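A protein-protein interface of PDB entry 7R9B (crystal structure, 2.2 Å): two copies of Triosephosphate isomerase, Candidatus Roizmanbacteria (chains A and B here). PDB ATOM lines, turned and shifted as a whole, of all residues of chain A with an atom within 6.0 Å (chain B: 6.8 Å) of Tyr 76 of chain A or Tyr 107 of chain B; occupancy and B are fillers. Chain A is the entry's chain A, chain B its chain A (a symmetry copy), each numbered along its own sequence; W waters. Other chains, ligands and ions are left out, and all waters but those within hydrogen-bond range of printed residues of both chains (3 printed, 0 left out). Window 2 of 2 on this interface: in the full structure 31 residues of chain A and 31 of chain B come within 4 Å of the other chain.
Of the 12 printed residues of chain A, 6 touch a printed residue of chain B. Printed residues of chain A that touch a printed residue of chain B: Tyr 76, Glu 78, Ala 80, Tyr 81, Glu 84 and Thr 86. Hydrophobic or aromatic side chains of chain A that line the printed part of chain B: Tyr 76, Ala 80 and Tyr 81. Of the 10 printed residues of chain B, 5 touch a printed residue of chain A. Hydrophobic or aromatic side chains of chain B within 4 Å of the printed part of chain A: Ala 10, Tyr 107 and Phe 108. Among the printed residues, Asp or Glu carboxylates within 4 Å of a Lys or Arg side-chain nitrogen of the other chain: Glu 84 of chain A with Arg 104 of chain B.
The guanidinium group (NE) of Arg 104 of chain B lies within salt-bridge range of the side-chain carboxylate (OE2) of Glu 110 of chain B (2.9 Å). OG of Ser 74 of chain A lies within hydrogen-bond range of N of Tyr 76 of chain A, at 3.0 Å. N of His 109 of chain B lies within hydrogen-bond range of O of Arg 104 of chain B (3.3 Å). OG of Ser 74 of chain A sits at hydrogen-bond distance from OE1 of Glu 84 of chain A.
Water W3 bridges OH of Tyr 76 of chain A (2.5 Å) and O of Tyr 107 of chain B (2.6 Å). Water W2 bridges OH of Tyr 107 of chain B (2.5 Å) and O of Ala 80 of chain A (2.7 Å). Water W1 bridges the side-chain hydroxyl of Thr 86 of chain A and the backbone carbonyl oxygen of Ala 10 of chain B.
O of Ala 80 of chain A sits close to OE1 of Glu 103 of chain B. OE2 of Glu 84 of chain A lies within salt-bridge range of NH2 of Arg 104 of chain B (2.8 Å).
Tyr 76 of chain A touches two residues of chain B. Tyr 107 of chain B touches three residues of chain A. Of the printed residues of chain B, Ala 80 of chain A touches Glu 103 (3.2 Å) and Tyr 107 (3.8 Å). Printed residues of chain B within 4 Å of Glu 78 of chain A: Ala 10. Of the printed residues of chain A, Glu 103 of chain B touches Ala 80 and Tyr 81. Printed residues of chain A within 4 Å of Ala 10 of chain B: Glu 78 (3.3 Å), Tyr 81 (3.6 Å), Glu 84 (3.96 Å) and Thr 86 (3.97 Å). Of the printed residues of chain A, Arg 104 of chain B touches Glu 84. Val 85 of chain A touches none of the printed residues of chain B. The nearest residue of chain B that does not touch Tyr 76 of chain A is Asp 106 of chain B (6.1 Å).
No position is printed for both chains. Of the 12 pairs that touch across the chains among the printed residues, none has its exchanged pair printed and touching as well.
Among the printed residues, pairs that only touch across the chains: Glu 84 of chain A with Phe 108 of chain B, Glu 78 of chain A with Ala 10 of chain B, Tyr 76 of chain A with Tyr 107 of chain B, Tyr 81 of chain A with Tyr 107 of chain B, Tyr 76 of chain A with Phe 108 of chain B, Tyr 81 of chain A with Ala 10 of chain B, Ala 80 of chain A with Tyr 107 of chain B, Tyr 81 of chain A with Glu 103 of chain B, Glu 84 of chain A with Ala 10 of chain B and Thr 86 of chain A with Ala 10 of chain B.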
ATOM      1  N   SER A  74      10.814  15.545  -2.046  1.00  0.00           N
ATOM      2  CA  SER A  74      10.406  16.886  -2.473  1.00  0.00           C
ATOM      3  C   SER A  74       9.077  16.862  -3.229  1.00  0.00           C
ATOM      4  O   SER A  74       8.763  15.912  -3.956  1.00  0.00           O
ATOM      5  CB  SER A  74      11.484  17.507  -3.369  1.00  0.00           C
ATOM      6  OG  SER A  74      11.200  18.870  -3.652  1.00  0.00           O
ATOM      7  N   VAL A  75       8.293  17.935  -3.066  1.00  0.00           N
ATOM      8  CA  VAL A  75       7.164  18.148  -3.973  1.00  0.00           C
ATOM      9  C   VAL A  75       7.624  18.506  -5.374  1.00  0.00           C
ATOM     10  O   VAL A  75       6.820  18.435  -6.310  1.00  0.00           O
ATOM     11  CB  VAL A  75       6.198  19.262  -3.526  1.00  0.00           C
ATOM     12  CG1 VAL A  75       5.510  18.892  -2.262  1.00  0.00           C
ATOM     13  CG2 VAL A  75       6.929  20.600  -3.397  1.00  0.00           C
ATOM     14  N   TYR A  76       8.886  18.897  -5.547  1.00  0.00           N
ATOM     15  CA  TYR A  76       9.415  19.300  -6.847  1.00  0.00           C
ATOM     16  C   TYR A  76      10.219  18.181  -7.499  1.00  0.00           C
ATOM     17  O   TYR A  76      10.735  17.274  -6.838  1.00  0.00           O
ATOM     18  CB  TYR A  76      10.306  20.544  -6.716  1.00  0.00           C
ATOM     19  CG  TYR A  76       9.548  21.754  -6.261  1.00  0.00           C
ATOM     20  CD1 TYR A  76       8.803  22.506  -7.166  1.00  0.00           C
ATOM     21  CD2 TYR A  76       9.552  22.143  -4.920  1.00  0.00           C
ATOM     22  CE1 TYR A  76       8.080  23.609  -6.752  1.00  0.00           C
ATOM     23  CE2 TYR A  76       8.815  23.261  -4.492  1.00  0.00           C
ATOM     24  CZ  TYR A  76       8.088  23.984  -5.422  1.00  0.00           C
ATOM     25  OH  TYR A  76       7.366  25.086  -5.037  1.00  0.00           O
ATOM     26  N   GLY A  77      10.320  18.268  -8.827  1.00  0.00           N
ATOM     27  CA  GLY A  77      11.246  17.463  -9.591  1.00  0.00           C
ATOM     28  C   GLY A  77      12.591  18.148  -9.682  1.00  0.00           C
ATOM     29  O   GLY A  77      12.880  19.108  -8.963  1.00  0.00           O
ATOM     30  N   GLU A  78      13.428  17.638 -10.589  1.00  0.00           N
ATOM     31  CA  GLU A  78      14.733  18.240 -10.840  1.00  0.00           C
ATOM     32  C   GLU A  78      14.571  19.722 -11.171  1.00  0.00           C
ATOM     33  O   GLU A  78      13.628  20.123 -11.858  1.00  0.00           O
ATOM     34  CB  GLU A  78      15.444  17.510 -11.988  1.00  0.00           C
ATOM     35  CG  GLU A  78      16.958  17.723 -12.041  1.00  0.00           C
ATOM     36  CD  GLU A  78      17.684  16.699 -12.920  1.00  0.00           C
ATOM     37  OE1 GLU A  78      16.990  15.956 -13.648  1.00  0.00           O
ATOM     38  OE2 GLU A  78      18.941  16.628 -12.879  1.00  0.00           O
ATOM     39  N   ALA A  80      15.960  24.089  -9.979  1.00  0.00           N
ATOM     40  CA  ALA A  80      16.626  25.049  -9.104  1.00  0.00           C
ATOM     41  C   ALA A  80      15.812  25.201  -7.819  1.00  0.00           C
ATOM     42  O   ALA A  80      15.105  26.184  -7.597  1.00  0.00           O
ATOM     43  CB  ALA A  80      16.807  26.380  -9.827  1.00  0.00           C
ATOM     44  N   TYR A  81      15.906  24.172  -6.964  1.00  0.00           N
ATOM     45  CA  TYR A  81      15.231  24.155  -5.654  1.00  0.00           C
ATOM     46  C   TYR A  81      16.271  23.782  -4.599  1.00  0.00           C
ATOM     47  O   TYR A  81      16.346  22.623  -4.178  1.00  0.00           O
ATOM     48  CB  TYR A  81      14.042  23.191  -5.657  1.00  0.00           C
ATOM     49  CG  TYR A  81      13.160  23.343  -6.881  1.00  0.00           C
ATOM     50  CD1 TYR A  81      12.332  24.453  -7.035  1.00  0.00           C
ATOM     51  CD2 TYR A  81      13.158  22.379  -7.880  1.00  0.00           C
ATOM     52  CE1 TYR A  81      11.526  24.597  -8.157  1.00  0.00           C
ATOM     53  CE2 TYR A  81      12.356  22.514  -9.012  1.00  0.00           C
ATOM     54  CZ  TYR A  81      11.547  23.619  -9.140  1.00  0.00           C
ATOM     55  OH  TYR A  81      10.759  23.737 -10.249  1.00  0.00           O
ATOM     56  N   GLU A  84      16.377  20.666  -1.770  1.00  0.00           N
ATOM     57  CA  GLU A  84      15.348  19.663  -1.985  1.00  0.00           C
ATOM     58  C   GLU A  84      15.969  18.336  -2.398  1.00  0.00           C
ATOM     59  O   GLU A  84      16.924  18.297  -3.182  1.00  0.00           O
ATOM     60  CB  GLU A  84      14.378  20.146  -3.066  1.00  0.00           C
ATOM     61  CG  GLU A  84      13.385  21.172  -2.577  1.00  0.00           C
ATOM     62  CD  GLU A  84      12.709  20.720  -1.273  1.00  0.00           C
ATOM     63  OE1 GLU A  84      11.806  19.838  -1.331  1.00  0.00           O
ATOM     64  OE2 GLU A  84      13.098  21.239  -0.197  1.00  0.00           O
ATOM     65  N   VAL A  85      15.404  17.244  -1.897  1.00  0.00           N
ATOM     66  CA  VAL A  85      15.776  15.904  -2.346  1.00  0.00           C
ATOM     67  C   VAL A  85      14.605  15.340  -3.141  1.00  0.00           C
ATOM     68  O   VAL A  85      13.502  15.168  -2.599  1.00  0.00           O
ATOM     69  CB  VAL A  85      16.165  15.002  -1.169  1.00  0.00           C
ATOM     70  CG1 VAL A  85      16.550  13.601  -1.674  1.00  0.00           C
ATOM     71  CG2 VAL A  85      17.311  15.634  -0.406  1.00  0.00           C
ATOM     72  N   THR A  86      14.838  15.082  -4.435  1.00  0.00           N
ATOM     73  CA  THR A  86      13.782  14.716  -5.367  1.00  0.00           C
ATOM     74  C   THR A  86      13.649  13.202  -5.461  1.00  0.00           C
ATOM     75  O   THR A  86      14.577  12.453  -5.153  1.00  0.00           O
ATOM     76  CB  THR A  86      14.047  15.274  -6.775  1.00  0.00           C
ATOM     77  OG1 THR A  86      15.254  14.704  -7.293  1.00  0.00           O
ATOM     78  CG2 THR A  86      14.141  16.815  -6.780  1.00  0.00           C
ATOM     79  N   ALA A  87      12.482  12.765  -5.939  1.00  0.00           N
ATOM     80  CA  ALA A  87      12.276  11.345  -6.213  1.00  0.00           C
ATOM     81  C   ALA A  87      13.334  10.803  -7.169  1.00  0.00           C
ATOM     82  O   ALA A  87      13.841   9.691  -6.978  1.00  0.00           O
ATOM     83  CB  ALA A  87      10.873  11.127  -6.783  1.00  0.00           C
ATOM     84  N   GLN A 121       5.413  12.378  -7.676  1.00  0.00           N
ATOM     85  CA  GLN A 121       6.849  12.348  -7.943  1.00  0.00           C
ATOM     86  C   GLN A 121       7.416  10.954  -7.706  1.00  0.00           C
ATOM     87  O   GLN A 121       8.210  10.448  -8.509  1.00  0.00           O
ATOM     88  CB  GLN A 121       7.578  13.370  -7.064  1.00  0.00           C
ATOM     89  CG  GLN A 121       7.221  14.824  -7.334  1.00  0.00           C
ATOM     90  CD  GLN A 121       7.775  15.308  -8.662  1.00  0.00           C
ATOM     91  OE1 GLN A 121       8.687  14.703  -9.213  1.00  0.00           O
ATOM     92  NE2 GLN A 121       7.236  16.413  -9.168  1.00  0.00           N
ATOM     93  N   ALA B  10      18.643  21.168  -6.893  1.00  0.00           N
ATOM     94  CA  ALA B  10      17.976  19.864  -6.914  1.00  0.00           C
ATOM     95  C   ALA B  10      18.291  19.123  -8.216  1.00  0.00           C
ATOM     96  O   ALA B  10      17.406  18.745  -8.982  1.00  0.00           O
ATOM     97  CB  ALA B  10      16.475  20.030  -6.709  1.00  0.00           C
ATOM     98  N   SER B 102      17.623  32.091  -1.331  1.00  0.00           N
ATOM     99  CA  SER B 102      16.442  32.768  -1.861  1.00  0.00           C
ATOM    100  C   SER B 102      15.371  31.793  -2.349  1.00  0.00           C
ATOM    101  O   SER B 102      14.171  32.048  -2.199  1.00  0.00           O
ATOM    102  CB  SER B 102      16.873  33.693  -2.995  1.00  0.00           C
ATOM    103  OG  SER B 102      15.741  34.231  -3.663  1.00  0.00           O
ATOM    104  N   GLU B 103      15.778  30.688  -2.965  1.00  0.00           N
ATOM    105  CA  GLU B 103      14.796  29.708  -3.408  1.00  0.00           C
ATOM    106  C   GLU B 103      13.995  29.146  -2.233  1.00  0.00           C
ATOM    107  O   GLU B 103      12.794  28.874  -2.366  1.00  0.00           O
ATOM    108  CB  GLU B 103      15.498  28.589  -4.180  1.00  0.00           C
ATOM    109  CG  GLU B 103      15.872  29.008  -5.606  1.00  0.00           C
ATOM    110  CD  GLU B 103      17.061  28.252  -6.174  1.00  0.00           C
ATOM    111  OE1 GLU B 103      17.533  27.275  -5.526  1.00  0.00           O
ATOM    112  OE2 GLU B 103      17.520  28.646  -7.276  1.00  0.00           O
ATOM    113  N   ARG B 104      14.618  28.981  -1.069  1.00  0.00           N
ATOM    114  CA  ARG B 104      13.850  28.482   0.068  1.00  0.00           C
ATOM    115  C   ARG B 104      12.899  29.548   0.607  1.00  0.00           C
ATOM    116  O   ARG B 104      11.856  29.210   1.179  1.00  0.00           O
ATOM    117  CB  ARG B 104      14.797  27.958   1.143  1.00  0.00           C
ATOM    118  CG  ARG B 104      15.659  26.813   0.593  1.00  0.00           C
ATOM    119  CD  ARG B 104      16.025  25.759   1.629  1.00  0.00           C
ATOM    120  NE  ARG B 104      14.854  25.126   2.225  1.00  0.00           N
ATOM    121  CZ  ARG B 104      14.228  24.054   1.737  1.00  0.00           C
ATOM    122  NH1 ARG B 104      13.167  23.572   2.387  1.00  0.00           N
ATOM    123  NH2 ARG B 104      14.644  23.469   0.603  1.00  0.00           N
ATOM    124  N   LYS B 105      13.214  30.834   0.407  1.00  0.00           N
ATOM    125  CA  LYS B 105      12.240  31.872   0.745  1.00  0.00           C
ATOM    126  C   LYS B 105      11.040  31.824  -0.196  1.00  0.00           C
ATOM    127  O   LYS B 105       9.893  31.900   0.257  1.00  0.00           O
ATOM    128  CB  LYS B 105      12.884  33.265   0.721  1.00  0.00           C
ATOM    129  CG  LYS B 105      14.264  33.350   1.365  1.00  0.00           C
ATOM    130  CD  LYS B 105      14.188  33.488   2.870  1.00  0.00           C
ATOM    131  CE  LYS B 105      15.592  33.471   3.506  1.00  0.00           C
ATOM    132  NZ  LYS B 105      16.331  34.703   3.155  1.00  0.00           N
ATOM    133  N   ASP B 106      11.283  31.672  -1.507  1.00  0.00           N
ATOM    134  CA  ASP B 106      10.191  31.699  -2.481  1.00  0.00           C
ATOM    135  C   ASP B 106       9.312  30.466  -2.377  1.00  0.00           C
ATOM    136  O   ASP B 106       8.083  30.574  -2.364  1.00  0.00           O
ATOM    137  CB  ASP B 106      10.728  31.807  -3.906  1.00  0.00           C
ATOM    138  CG  ASP B 106      11.389  33.127  -4.179  1.00  0.00           C
ATOM    139  OD1 ASP B 106      11.238  34.065  -3.358  1.00  0.00           O
ATOM    140  OD2 ASP B 106      12.078  33.218  -5.216  1.00  0.00           O
ATOM    141  N   TYR B 107       9.920  29.281  -2.337  1.00  0.00           N
ATOM    142  CA  TYR B 107       9.160  28.046  -2.467  1.00  0.00           C
ATOM    143  C   TYR B 107       8.710  27.461  -1.139  1.00  0.00           C
ATOM    144  O   TYR B 107       7.675  26.783  -1.098  1.00  0.00           O
ATOM    145  CB  TYR B 107       9.985  27.002  -3.217  1.00  0.00           C
ATOM    146  CG  TYR B 107      10.352  27.453  -4.595  1.00  0.00           C
ATOM    147  CD1 TYR B 107       9.379  27.873  -5.484  1.00  0.00           C
ATOM    148  CD2 TYR B 107      11.671  27.477  -5.007  1.00  0.00           C
ATOM    149  CE1 TYR B 107       9.710  28.298  -6.760  1.00  0.00           C
ATOM    150  CE2 TYR B 107      12.015  27.899  -6.274  1.00  0.00           C
ATOM    151  CZ  TYR B 107      11.032  28.304  -7.148  1.00  0.00           C
ATOM    152  OH  TYR B 107      11.385  28.726  -8.411  1.00  0.00           O
ATOM    153  N   PHE B 108       9.460  27.676  -0.056  1.00  0.00           N
ATOM    154  CA  PHE B 108       9.111  27.095   1.235  1.00  0.00           C
ATOM    155  C   PHE B 108       8.890  28.159   2.301  1.00  0.00           C
ATOM    156  O   PHE B 108       8.899  27.848   3.494  1.00  0.00           O
ATOM    157  CB  PHE B 108      10.175  26.072   1.639  1.00  0.00           C
ATOM    158  CG  PHE B 108      10.415  25.042   0.566  1.00  0.00           C
ATOM    159  CD1 PHE B 108       9.580  23.934   0.457  1.00  0.00           C
ATOM    160  CD2 PHE B 108      11.414  25.216  -0.368  1.00  0.00           C
ATOM    161  CE1 PHE B 108       9.759  23.007  -0.549  1.00  0.00           C
ATOM    162  CE2 PHE B 108      11.603  24.294  -1.381  1.00  0.00           C
ATOM    163  CZ  PHE B 108      10.762  23.195  -1.481  1.00  0.00           C
ATOM    164  N   HIS B 109       8.672  29.409   1.878  1.00  0.00           N
ATOM    165  CA  HIS B 109       8.269  30.517   2.757  1.00  0.00           C
ATOM    166  C   HIS B 109       9.163  30.622   3.997  1.00  0.00           C
ATOM    167  O   HIS B 109       8.704  30.961   5.088  1.00  0.00           O
ATOM    168  CB  HIS B 109       6.790  30.392   3.146  1.00  0.00           C
ATOM    169  N   GLU B 110      10.457  30.332   3.831  1.00  0.00           N
ATOM    170  CA  GLU B 110      11.396  30.574   4.914  1.00  0.00           C
ATOM    171  C   GLU B 110      11.470  32.070   5.204  1.00  0.00           C
ATOM    172  O   GLU B 110      11.486  32.900   4.291  1.00  0.00           O
ATOM    173  CB  GLU B 110      12.781  30.014   4.574  1.00  0.00           C
ATOM    174  CG  GLU B 110      12.826  28.480   4.532  1.00  0.00           C
ATOM    175  CD  GLU B 110      14.236  27.924   4.593  1.00  0.00           C
ATOM    176  OE1 GLU B 110      15.200  28.721   4.588  1.00  0.00           O
ATOM    177  OE2 GLU B 110      14.388  26.684   4.659  1.00  0.00           O
HETATM  178  O   HOH W   1      16.791  15.911  -9.142  1.00  0.00           O
HETATM  179  O   HOH W   2      13.747  28.132  -8.919  1.00  0.00           O
HETATM  180  O   HOH W   3       6.296  25.473  -2.830  1.00  0.00           O
